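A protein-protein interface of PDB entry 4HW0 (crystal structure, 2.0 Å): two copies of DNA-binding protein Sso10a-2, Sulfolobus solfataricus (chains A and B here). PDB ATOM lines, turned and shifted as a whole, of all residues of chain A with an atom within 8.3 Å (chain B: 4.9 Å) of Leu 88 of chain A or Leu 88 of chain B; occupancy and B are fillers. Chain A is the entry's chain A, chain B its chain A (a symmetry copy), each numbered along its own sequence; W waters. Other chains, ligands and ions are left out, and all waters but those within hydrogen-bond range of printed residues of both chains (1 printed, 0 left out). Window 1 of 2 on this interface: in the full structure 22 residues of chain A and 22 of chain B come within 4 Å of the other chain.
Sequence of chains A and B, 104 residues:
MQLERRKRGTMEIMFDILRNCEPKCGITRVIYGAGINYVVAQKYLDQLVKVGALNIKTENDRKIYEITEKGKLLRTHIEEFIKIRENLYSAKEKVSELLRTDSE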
ATOM      1  N   MET A  11      -0.213 -14.454 -12.571  1.00  0.00           N
ATOM      2  CA  MET A  11      -1.618 -14.119 -12.411  1.00  0.00           C
ATOM      3  C   MET A  11      -1.664 -12.658 -12.003  1.00  0.00           C
ATOM      4  O   MET A  11      -2.400 -11.816 -12.542  1.00  0.00           O
ATOM      5  CB  MET A  11      -2.412 -15.031 -11.432  1.00  0.00           C
ATOM      6  CG  MET A  11      -2.836 -16.280 -12.193  1.00  0.00           C
ATOM      7  SD  MET A  11      -3.904 -17.366 -10.929  1.00  0.00           S
ATOM      8  CE  MET A  11      -4.019 -19.033 -12.048  1.00  0.00           C
ATOM      9  N   HIS A  77     -11.678 -12.341 -11.442  1.00  0.00           N
ATOM     10  CA  HIS A  77     -11.262 -13.602 -10.819  1.00  0.00           C
ATOM     11  C   HIS A  77      -9.872 -13.584 -10.231  1.00  0.00           C
ATOM     12  O   HIS A  77      -9.648 -14.183  -9.163  1.00  0.00           O
ATOM     13  CB  HIS A  77     -11.396 -14.738 -11.791  1.00  0.00           C
ATOM     14  CG  HIS A  77     -12.799 -15.028 -12.151  1.00  0.00           C
ATOM     15  ND1 HIS A  77     -13.873 -14.671 -11.383  1.00  0.00           N
ATOM     16  CD2 HIS A  77     -13.313 -15.626 -13.233  1.00  0.00           C
ATOM     17  CE1 HIS A  77     -14.991 -15.034 -11.974  1.00  0.00           C
ATOM     18  NE2 HIS A  77     -14.673 -15.584 -13.119  1.00  0.00           N
ATOM     19  N   ILE A  78      -8.951 -12.918 -10.907  1.00  0.00           N
ATOM     20  CA  ILE A  78      -7.614 -12.783 -10.330  1.00  0.00           C
ATOM     21  C   ILE A  78      -7.705 -11.968  -9.061  1.00  0.00           C
ATOM     22  O   ILE A  78      -7.043 -12.268  -8.070  1.00  0.00           O
ATOM     23  CB  ILE A  78      -6.581 -12.229 -11.285  1.00  0.00           C
ATOM     24  CG1 ILE A  78      -6.406 -13.093 -12.526  1.00  0.00           C
ATOM     25  CG2 ILE A  78      -5.254 -12.205 -10.609  1.00  0.00           C
ATOM     26  CD1 ILE A  78      -5.578 -12.503 -13.658  1.00  0.00           C
ATOM     27  N   GLU A  80     -10.087 -11.738  -6.958  1.00  0.00           N
ATOM     28  CA  GLU A  80     -10.664 -12.606  -5.941  1.00  0.00           C
ATOM     29  C   GLU A  80      -9.606 -13.592  -5.418  1.00  0.00           C
ATOM     30  O   GLU A  80      -9.457 -13.766  -4.199  1.00  0.00           O
ATOM     31  CB  GLU A  80     -11.954 -13.203  -6.465  1.00  0.00           C
ATOM     32  CG  GLU A  80     -12.620 -14.138  -5.467  1.00  0.00           C
ATOM     33  CD  GLU A  80     -13.176 -13.446  -4.179  1.00  0.00           C
ATOM     34  OE1 GLU A  80     -13.046 -12.201  -4.033  1.00  0.00           O
ATOM     35  OE2 GLU A  80     -13.798 -14.175  -3.343  1.00  0.00           O
ATOM     36  N   PHE A  81      -8.785 -14.157  -6.325  1.00  0.00           N
ATOM     37  CA  PHE A  81      -7.663 -15.041  -5.943  1.00  0.00           C
ATOM     38  C   PHE A  81      -6.683 -14.337  -5.004  1.00  0.00           C
ATOM     39  O   PHE A  81      -6.261 -14.870  -3.964  1.00  0.00           O
ATOM     40  CB  PHE A  81      -6.955 -15.612  -7.196  1.00  0.00           C
ATOM     41  CG  PHE A  81      -5.671 -16.307  -6.898  1.00  0.00           C
ATOM     42  CD1 PHE A  81      -4.473 -15.577  -6.782  1.00  0.00           C
ATOM     43  CD2 PHE A  81      -5.638 -17.645  -6.677  1.00  0.00           C
ATOM     44  CE1 PHE A  81      -3.292 -16.219  -6.462  1.00  0.00           C
ATOM     45  CE2 PHE A  81      -4.457 -18.292  -6.379  1.00  0.00           C
ATOM     46  CZ  PHE A  81      -3.275 -17.572  -6.243  1.00  0.00           C
ATOM     47  N   ILE A  82      -6.337 -13.122  -5.370  1.00  0.00           N
ATOM     48  CA  ILE A  82      -5.364 -12.365  -4.586  1.00  0.00           C
ATOM     49  C   ILE A  82      -5.839 -12.062  -3.179  1.00  0.00           C
ATOM     50  O   ILE A  82      -5.124 -12.242  -2.195  1.00  0.00           O
ATOM     51  CB  ILE A  82      -4.997 -11.080  -5.354  1.00  0.00           C
ATOM     52  CG1 ILE A  82      -4.130 -11.445  -6.545  1.00  0.00           C
ATOM     53  CG2 ILE A  82      -4.291 -10.069  -4.449  1.00  0.00           C
ATOM     54  CD1 ILE A  82      -4.010 -10.296  -7.520  1.00  0.00           C
ATOM     55  N   LYS A  83      -7.077 -11.657  -3.080  1.00  0.00           N
ATOM     56  CA  LYS A  83      -7.677 -11.351  -1.827  1.00  0.00           C
ATOM     57  C   LYS A  83      -7.763 -12.614  -0.932  1.00  0.00           C
ATOM     58  O   LYS A  83      -7.412 -12.576   0.225  1.00  0.00           O
ATOM     59  CB  LYS A  83      -9.058 -10.738  -2.083  1.00  0.00           C
ATOM     60  CG  LYS A  83     -10.012 -10.732  -0.911  1.00  0.00           C
ATOM     61  CD  LYS A  83     -11.420 -10.333  -1.333  1.00  0.00           C
ATOM     62  CE  LYS A  83     -12.490 -11.118  -0.598  1.00  0.00           C
ATOM     63  NZ  LYS A  83     -13.797 -11.040  -1.329  1.00  0.00           N
ATOM     64  N   ILE A  84      -8.189 -13.739  -1.470  1.00  0.00           N
ATOM     65  CA  ILE A  84      -8.196 -14.975  -0.667  1.00  0.00           C
ATOM     66  C   ILE A  84      -6.789 -15.397  -0.249  1.00  0.00           C
ATOM     67  O   ILE A  84      -6.570 -15.896   0.855  1.00  0.00           O
ATOM     68  CB  ILE A  84      -8.874 -16.139  -1.453  1.00  0.00           C
ATOM     69  CG1 ILE A  84     -10.359 -15.789  -1.687  1.00  0.00           C
ATOM     70  CG2 ILE A  84      -8.800 -17.428  -0.663  1.00  0.00           C
ATOM     71  CD1 ILE A  84     -11.071 -16.614  -2.742  1.00  0.00           C
ATOM     72  N   ARG A  85      -5.819 -15.213  -1.139  1.00  0.00           N
ATOM     73  CA  ARG A  85      -4.454 -15.578  -0.826  1.00  0.00           C
ATOM     74  C   ARG A  85      -3.949 -14.767   0.357  1.00  0.00           C
ATOM     75  O   ARG A  85      -3.205 -15.290   1.208  1.00  0.00           O
ATOM     76  CB  ARG A  85      -3.542 -15.386  -2.032  1.00  0.00           C
ATOM     77  CG  ARG A  85      -2.105 -15.856  -1.834  1.00  0.00           C
ATOM     78  CD  ARG A  85      -1.251 -15.567  -3.058  1.00  0.00           C
ATOM     79  NE  ARG A  85      -1.169 -14.116  -3.268  1.00  0.00           N
ATOM     80  CZ  ARG A  85      -0.568 -13.536  -4.299  1.00  0.00           C
ATOM     81  NH1 ARG A  85       0.036 -14.277  -5.235  1.00  0.00           N
ATOM     82  NH2 ARG A  85      -0.574 -12.217  -4.375  1.00  0.00           N
ATOM     83  N   GLU A  86      -4.326 -13.496   0.406  1.00  0.00           N
ATOM     84  CA  GLU A  86      -3.960 -12.664   1.535  1.00  0.00           C
ATOM     85  C   GLU A  86      -4.562 -13.208   2.808  1.00  0.00           C
ATOM     86  O   GLU A  86      -3.924 -13.180   3.846  1.00  0.00           O
ATOM     87  CB  GLU A  86      -4.453 -11.176   1.355  1.00  0.00           C
ATOM     88  CG  GLU A  86      -3.520 -10.343   0.456  1.00  0.00           C
ATOM     89  CD  GLU A  86      -2.027 -10.412   0.928  1.00  0.00           C
ATOM     90  OE1 GLU A  86      -1.803 -10.070   2.116  1.00  0.00           O
ATOM     91  OE2 GLU A  86      -1.084 -10.861   0.176  1.00  0.00           O
ATOM     92  N   ASN A  87      -5.828 -13.587   2.761  1.00  0.00           N
ATOM     93  CA  ASN A  87      -6.507 -14.162   3.926  1.00  0.00           C
ATOM     94  C   ASN A  87      -5.840 -15.455   4.395  1.00  0.00           C
ATOM     95  O   ASN A  87      -5.752 -15.684   5.563  1.00  0.00           O
ATOM     96  CB  ASN A  87      -7.961 -14.447   3.637  1.00  0.00           C
ATOM     97  CG  ASN A  87      -8.762 -13.181   3.441  1.00  0.00           C
ATOM     98  OD1 ASN A  87      -8.343 -12.096   3.853  1.00  0.00           O
ATOM     99  ND2 ASN A  87      -9.897 -13.306   2.775  1.00  0.00           N
ATOM    100  N   LEU A  88      -5.388 -16.264   3.460  1.00  0.00           N
ATOM    101  CA  LEU A  88      -4.617 -17.463   3.764  1.00  0.00           C
ATOM    102  C   LEU A  88      -3.308 -17.168   4.497  1.00  0.00           C
ATOM    103  O   LEU A  88      -3.026 -17.804   5.487  1.00  0.00           O
ATOM    104  CB  LEU A  88      -4.331 -18.238   2.487  1.00  0.00           C
ATOM    105  CG  LEU A  88      -3.737 -19.596   2.763  1.00  0.00           C
ATOM    106  CD1 LEU A  88      -4.828 -20.519   3.321  1.00  0.00           C
ATOM    107  CD2 LEU A  88      -3.207 -20.166   1.467  1.00  0.00           C
ATOM    108  N   TYR A  89      -2.559 -16.173   4.043  1.00  0.00           N
ATOM    109  CA  TYR A  89      -1.352 -15.773   4.794  1.00  0.00           C
ATOM    110  C   TYR A  89      -1.672 -15.392   6.208  1.00  0.00           C
ATOM    111  O   TYR A  89      -1.002 -15.820   7.131  1.00  0.00           O
ATOM    112  CB  TYR A  89      -0.581 -14.583   4.195  1.00  0.00           C
ATOM    113  CG  TYR A  89       0.005 -14.720   2.792  1.00  0.00           C
ATOM    114  CD1 TYR A  89       0.451 -15.947   2.275  1.00  0.00           C
ATOM    115  CD2 TYR A  89       0.135 -13.563   1.965  1.00  0.00           C
ATOM    116  CE1 TYR A  89       0.993 -16.022   0.988  1.00  0.00           C
ATOM    117  CE2 TYR A  89       0.658 -13.639   0.674  1.00  0.00           C
ATOM    118  CZ  TYR A  89       1.099 -14.864   0.199  1.00  0.00           C
ATOM    119  OH  TYR A  89       1.617 -14.902  -1.082  1.00  0.00           O
ATOM    120  N   SER A  90      -2.693 -14.570   6.404  1.00  0.00           N
ATOM    121  CA  SER A  90      -3.081 -14.180   7.751  1.00  0.00           C
ATOM    122  C   SER A  90      -3.479 -15.355   8.596  1.00  0.00           C
ATOM    123  O   SER A  90      -3.154 -15.398   9.750  1.00  0.00           O
ATOM    124  CB  SER A  90      -4.240 -13.182   7.773  1.00  0.00           C
ATOM    125  OG  SER A  90      -3.815 -12.018   7.042  1.00  0.00           O
ATOM    126  N   ALA A  91      -4.294 -16.264   8.030  1.00  0.00           N
ATOM    127  CA  ALA A  91      -4.733 -17.459   8.756  1.00  0.00           C
ATOM    128  C   ALA A  91      -3.551 -18.348   9.158  1.00  0.00           C
ATOM    129  O   ALA A  91      -3.473 -18.842  10.278  1.00  0.00           O
ATOM    130  CB  ALA A  91      -5.746 -18.214   7.925  1.00  0.00           C
ATOM    131  N   LYS A  92      -2.578 -18.456   8.269  1.00  0.00           N
ATOM    132  CA  LYS A  92      -1.340 -19.194   8.583  1.00  0.00           C
ATOM    133  C   LYS A  92      -0.560 -18.557   9.718  1.00  0.00           C
ATOM    134  O   LYS A  92      -0.131 -19.237  10.658  1.00  0.00           O
ATOM    135  CB  LYS A  92      -0.475 -19.319   7.353  1.00  0.00           C
ATOM    136  CG  LYS A  92       0.783 -20.181   7.520  1.00  0.00           C
ATOM    137  CD  LYS A  92       1.213 -20.656   6.139  1.00  0.00           C
ATOM    138  CE  LYS A  92       2.284 -21.752   6.121  1.00  0.00           C
ATOM    139  NZ  LYS A  92       3.426 -21.471   7.050  1.00  0.00           N
ATOM    140  N   GLU A  93      -0.464 -17.231   9.697  1.00  0.00           N
ATOM    141  CA  GLU A  93       0.214 -16.502  10.784  1.00  0.00           C
ATOM    142  C   GLU A  93      -0.487 -16.744  12.106  1.00  0.00           C
ATOM    143  O   GLU A  93       0.153 -16.863  13.132  1.00  0.00           O
ATOM    144  CB  GLU A  93       0.266 -14.969  10.532  1.00  0.00           C
ATOM    145  CG  GLU A  93       1.177 -14.502   9.397  1.00  0.00           C
ATOM    146  CD  GLU A  93       0.921 -13.020   8.959  1.00  0.00           C
ATOM    147  OE1 GLU A  93       0.131 -12.266   9.615  1.00  0.00           O
ATOM    148  OE2 GLU A  93       1.489 -12.611   7.911  1.00  0.00           O
ATOM    149  N   LYS A  94      -1.806 -16.804  12.088  1.00  0.00           N
ATOM    150  CA  LYS A  94      -2.534 -17.038  13.337  1.00  0.00           C
ATOM    151  C   LYS A  94      -2.261 -18.421  13.921  1.00  0.00           C
ATOM    152  O   LYS A  94      -2.173 -18.598  15.123  1.00  0.00           O
ATOM    153  CB  LYS A  94      -4.050 -16.892  13.167  1.00  0.00           C
ATOM    154  CG  LYS A  94      -4.570 -15.507  12.946  1.00  0.00           C
ATOM    155  CD  LYS A  94      -6.107 -15.519  13.127  1.00  0.00           C
ATOM    156  CE  LYS A  94      -6.501 -15.176  14.582  1.00  0.00           C
ATOM    157  NZ  LYS A  94      -7.995 -15.050  14.692  1.00  0.00           N
ATOM    158  N   VAL A  95      -2.126 -19.412  13.056  1.00  0.00           N
ATOM    159  CA  VAL A  95      -1.715 -20.743  13.515  1.00  0.00           C
ATOM    160  C   VAL A  95      -0.302 -20.691  14.092  1.00  0.00           C
ATOM    161  O   VAL A  95      -0.012 -21.169  15.182  1.00  0.00           O
ATOM    162  CB  VAL A  95      -1.737 -21.745  12.344  1.00  0.00           C
ATOM    163  CG1 VAL A  95      -1.143 -23.070  12.779  1.00  0.00           C
ATOM    164  CG2 VAL A  95      -3.152 -21.886  11.837  1.00  0.00           C
ATOM    165  N   PHE B  81      -7.676 -22.097   8.364  1.00  0.00           N
ATOM    166  CA  PHE B  81      -6.626 -22.129   7.324  1.00  0.00           C
ATOM    167  C   PHE B  81      -6.979 -23.098   6.195  1.00  0.00           C
ATOM    168  O   PHE B  81      -6.880 -22.784   4.996  1.00  0.00           O
ATOM    169  CB  PHE B  81      -5.241 -22.440   7.942  1.00  0.00           C
ATOM    170  CG  PHE B  81      -4.183 -22.733   6.934  1.00  0.00           C
ATOM    171  CD1 PHE B  81      -4.035 -24.030   6.409  1.00  0.00           C
ATOM    172  CD2 PHE B  81      -3.382 -21.747   6.460  1.00  0.00           C
ATOM    173  CE1 PHE B  81      -3.083 -24.288   5.442  1.00  0.00           C
ATOM    174  CE2 PHE B  81      -2.416 -22.005   5.510  1.00  0.00           C
ATOM    175  CZ  PHE B  81      -2.279 -23.281   4.974  1.00  0.00           C
ATOM    176  N   ILE B  84      -9.931 -21.816   4.013  1.00  0.00           N
ATOM    177  CA  ILE B  84      -9.498 -20.759   3.080  1.00  0.00           C
ATOM    178  C   ILE B  84      -8.608 -21.306   1.966  1.00  0.00           C
ATOM    179  O   ILE B  84      -8.678 -20.870   0.817  1.00  0.00           O
ATOM    180  CB  ILE B  84      -8.739 -19.629   3.842  1.00  0.00           C
ATOM    181  CG1 ILE B  84      -9.714 -18.943   4.822  1.00  0.00           C
ATOM    182  CG2 ILE B  84      -8.219 -18.592   2.872  1.00  0.00           C
ATOM    183  CD1 ILE B  84      -9.071 -18.088   5.898  1.00  0.00           C
ATOM    184  N   ARG B  85      -7.748 -22.261   2.300  1.00  0.00           N
ATOM    185  CA  ARG B  85      -6.870 -22.843   1.307  1.00  0.00           C
ATOM    186  C   ARG B  85      -7.683 -23.523   0.218  1.00  0.00           C
ATOM    187  O   ARG B  85      -7.314 -23.469  -0.971  1.00  0.00           O
ATOM    188  CB  ARG B  85      -5.897 -23.830   1.941  1.00  0.00           C
ATOM    189  CG  ARG B  85      -4.853 -24.405   0.990  1.00  0.00           C
ATOM    190  CD  ARG B  85      -3.969 -25.427   1.687  1.00  0.00           C
ATOM    191  NE  ARG B  85      -4.784 -26.568   2.120  1.00  0.00           N
ATOM    192  CZ  ARG B  85      -4.332 -27.593   2.831  1.00  0.00           C
ATOM    193  NH1 ARG B  85      -3.044 -27.649   3.193  1.00  0.00           N
ATOM    194  NH2 ARG B  85      -5.175 -28.554   3.165  1.00  0.00           N
ATOM    195  N   GLU B  86      -8.767 -24.178   0.612  1.00  0.00           N
ATOM    196  CA  GLU B  86      -9.649 -24.793  -0.360  1.00  0.00           C
ATOM    197  C   GLU B  86     -10.242 -23.745  -1.271  1.00  0.00           C
ATOM    198  O   GLU B  86     -10.390 -23.980  -2.457  1.00  0.00           O
ATOM    199  CB  GLU B  86     -10.834 -25.574   0.329  1.00  0.00           C
ATOM    200  CG  GLU B  86     -10.422 -26.974   0.819  1.00  0.00           C
ATOM    201  CD  GLU B  86      -9.742 -27.820  -0.311  1.00  0.00           C
ATOM    202  OE1 GLU B  86     -10.408 -27.976  -1.366  1.00  0.00           O
ATOM    203  OE2 GLU B  86      -8.543 -28.275  -0.209  1.00  0.00           O
ATOM    204  N   ASN B  87     -10.696 -22.641  -0.702  1.00  0.00           N
ATOM    205  CA  ASN B  87     -11.261 -21.541  -1.490  1.00  0.00           C
ATOM    206  C   ASN B  87     -10.243 -20.959  -2.470  1.00  0.00           C
ATOM    207  O   ASN B  87     -10.598 -20.617  -3.557  1.00  0.00           O
ATOM    208  CB  ASN B  87     -11.770 -20.429  -0.606  1.00  0.00           C
ATOM    209  CG  ASN B  87     -12.978 -20.847   0.200  1.00  0.00           C
ATOM    210  OD1 ASN B  87     -13.654 -21.824  -0.134  1.00  0.00           O
ATOM    211  ND2 ASN B  87     -13.229 -20.139   1.287  1.00  0.00           N
ATOM    212  N   LEU B  88      -8.999 -20.865  -2.049  1.00  0.00           N
ATOM    213  CA  LEU B  88      -7.905 -20.453  -2.919  1.00  0.00           C
ATOM    214  C   LEU B  88      -7.698 -21.386  -4.113  1.00  0.00           C
ATOM    215  O   LEU B  88      -7.587 -20.916  -5.221  1.00  0.00           O
ATOM    216  CB  LEU B  88      -6.616 -20.341  -2.120  1.00  0.00           C
ATOM    217  CG  LEU B  88      -5.504 -19.702  -2.913  1.00  0.00           C
ATOM    218  CD1 LEU B  88      -5.785 -18.201  -3.055  1.00  0.00           C
ATOM    219  CD2 LEU B  88      -4.201 -19.905  -2.174  1.00  0.00           C
ATOM    220  N   TYR B  89      -7.712 -22.691  -3.881  1.00  0.00           N
ATOM    221  CA  TYR B  89      -7.642 -23.630  -5.020  1.00  0.00           C
ATOM    222  C   TYR B  89      -8.754 -23.407  -5.999  1.00  0.00           C
ATOM    223  O   TYR B  89      -8.525 -23.357  -7.195  1.00  0.00           O
ATOM    224  CB  TYR B  89      -7.703 -25.120  -4.636  1.00  0.00           C
ATOM    225  CG  TYR B  89      -6.604 -25.693  -3.745  1.00  0.00           C
ATOM    226  CD1 TYR B  89      -5.286 -25.209  -3.763  1.00  0.00           C
ATOM    227  CD2 TYR B  89      -6.902 -26.779  -2.866  1.00  0.00           C
ATOM    228  CE1 TYR B  89      -4.309 -25.775  -2.936  1.00  0.00           C
ATOM    229  CE2 TYR B  89      -5.934 -27.331  -2.027  1.00  0.00           C
ATOM    230  CZ  TYR B  89      -4.640 -26.838  -2.079  1.00  0.00           C
ATOM    231  OH  TYR B  89      -3.706 -27.412  -1.239  1.00  0.00           O
ATOM    232  N   SER B  90      -9.981 -23.281  -5.513  1.00  0.00           N
ATOM    233  CA  SER B  90     -11.107 -23.032  -6.401  1.00  0.00           C
ATOM    234  C   SER B  90     -10.959 -21.752  -7.170  1.00  0.00           C
ATOM    235  O   SER B  90     -11.295 -21.704  -8.321  1.00  0.00           O
ATOM    236  CB  SER B  90     -12.447 -22.977  -5.664  1.00  0.00           C
ATOM    237  OG  SER B  90     -12.626 -24.245  -5.008  1.00  0.00           O
ATOM    238  N   ALA B  91     -10.554 -20.671  -6.479  1.00  0.00           N
ATOM    239  CA  ALA B  91     -10.360 -19.372  -7.131  1.00  0.00           C
ATOM    240  C   ALA B  91      -9.281 -19.437  -8.219  1.00  0.00           C
ATOM    241  O   ALA B  91      -9.444 -18.906  -9.314  1.00  0.00           O
ATOM    242  CB  ALA B  91     -10.043 -18.324  -6.089  1.00  0.00           C
ATOM    243  N   LYS B  92      -8.226 -20.184  -7.946  1.00  0.00           N
ATOM    244  CA  LYS B  92      -7.174 -20.411  -8.954  1.00  0.00           C
ATOM    245  C   LYS B  92      -7.691 -21.159 -10.169  1.00  0.00           C
ATOM    246  O   LYS B  92      -7.441 -20.765 -11.315  1.00  0.00           O
ATOM    247  CB  LYS B  92      -6.005 -21.143  -8.341  1.00  0.00           C
ATOM    248  CG  LYS B  92      -4.789 -21.325  -9.259  1.00  0.00           C
ATOM    249  CD  LYS B  92      -3.567 -21.546  -8.379  1.00  0.00           C
ATOM    250  CE  LYS B  92      -2.215 -21.471  -9.097  1.00  0.00           C
ATOM    251  NZ  LYS B  92      -2.188 -22.245 -10.379  1.00  0.00           N
HETATM  252  O   HOH W   1     -11.036 -16.592  -8.800  1.00  0.00           O
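Phe 81 of chain A touches Leu 88 of chain B, and with the chains exchanged Leu 88 of chain A touches Phe 81 of chain B.
Ile 84 of chain A touches Leu 88 of chain B, and with the chains exchanged Leu 88 of chain A touches Ile 84 of chain B.
Ile 84 of chain A touches Ala 91 of chain B, and with the chains exchanged Ala 91 of chain A touches Ile 84 of chain B.
Leu 88 of chain B touches its own counterpart, Leu 88 of chain A.
Of the 13 pairs that touch across the chains among the printed residues, 12 have their exchanged pair printed and touching as well.
Of the 10 printed residues of chain B, 6 touch a printed residue of chain A.
Hydrophobic or aromatic side chains of chain B that line the printed part of chain A: Phe 81, Ile 84, Leu 88 and Ala 91.
Among the printed residues, 13 pairs touch across the chains.
Among the printed residues, no Asp or Glu carboxylate lies within 4 Å of a Lys or Arg side-chain nitrogen of the other chain.
Leu 88 of chain B touches Phe 81 of chain A.
CB of Lys 92 of chain B touches CE2 of Phe 81 of chain A (3.8 Å).
Ile 84 of chain A touches Ile 84 of chain B (CG2 to O, 3.7 Å).
Ala 91 of chain B touches Ile 84 of chain A (CB to CD1, 3.9 Å).
Arg 85 of chain A touches Leu 88 of chain B.
Phe 81 of chain B touches Leu 88 of chain A (O to CD1, 3.5 Å).
Ile 84 of chain B touches Leu 88 of chain A (CG2 to N, 3.7 Å).
N of Arg 85 of chain B touches CD1 of Leu 88 of chain A, at 3.6 Å.
Leu 88 of chain B touches Leu 88 of chain A.
CE2 of Phe 81 of chain B touches CB of Lys 92 of chain A, 3.8 Å away.
Printed residues of chain B within 4 Å of Met 11 of chain A: Lys 92.
Of the printed residues of chain B, Phe 81 of chain A touches Leu 88 (3.5 Å) and Lys 92 (3.8 Å).
Leu 88 of chain A touches four residues of chain B.
Of the printed residues of chain B, Ala 91 of chain A touches Ile 84.
Printed residues of chain A within 4 Å of Arg 85 of chain B: Leu 88.
Of chain A, only Phe 81 (3.5 Å), Ile 84 (3.7 Å), Arg 85 (3.5 Å) and Leu 88 (3.8 Å) come within 4 Å of Leu 88 of chain B.
The nearest printed residue of chain B that does not touch Lys 92 of chain A is Ile 84 of chain B (6.9 Å).
Water W1 lies within hydrogen-bond range of O of His 77 of chain A and O of Ala 91 of chain B.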
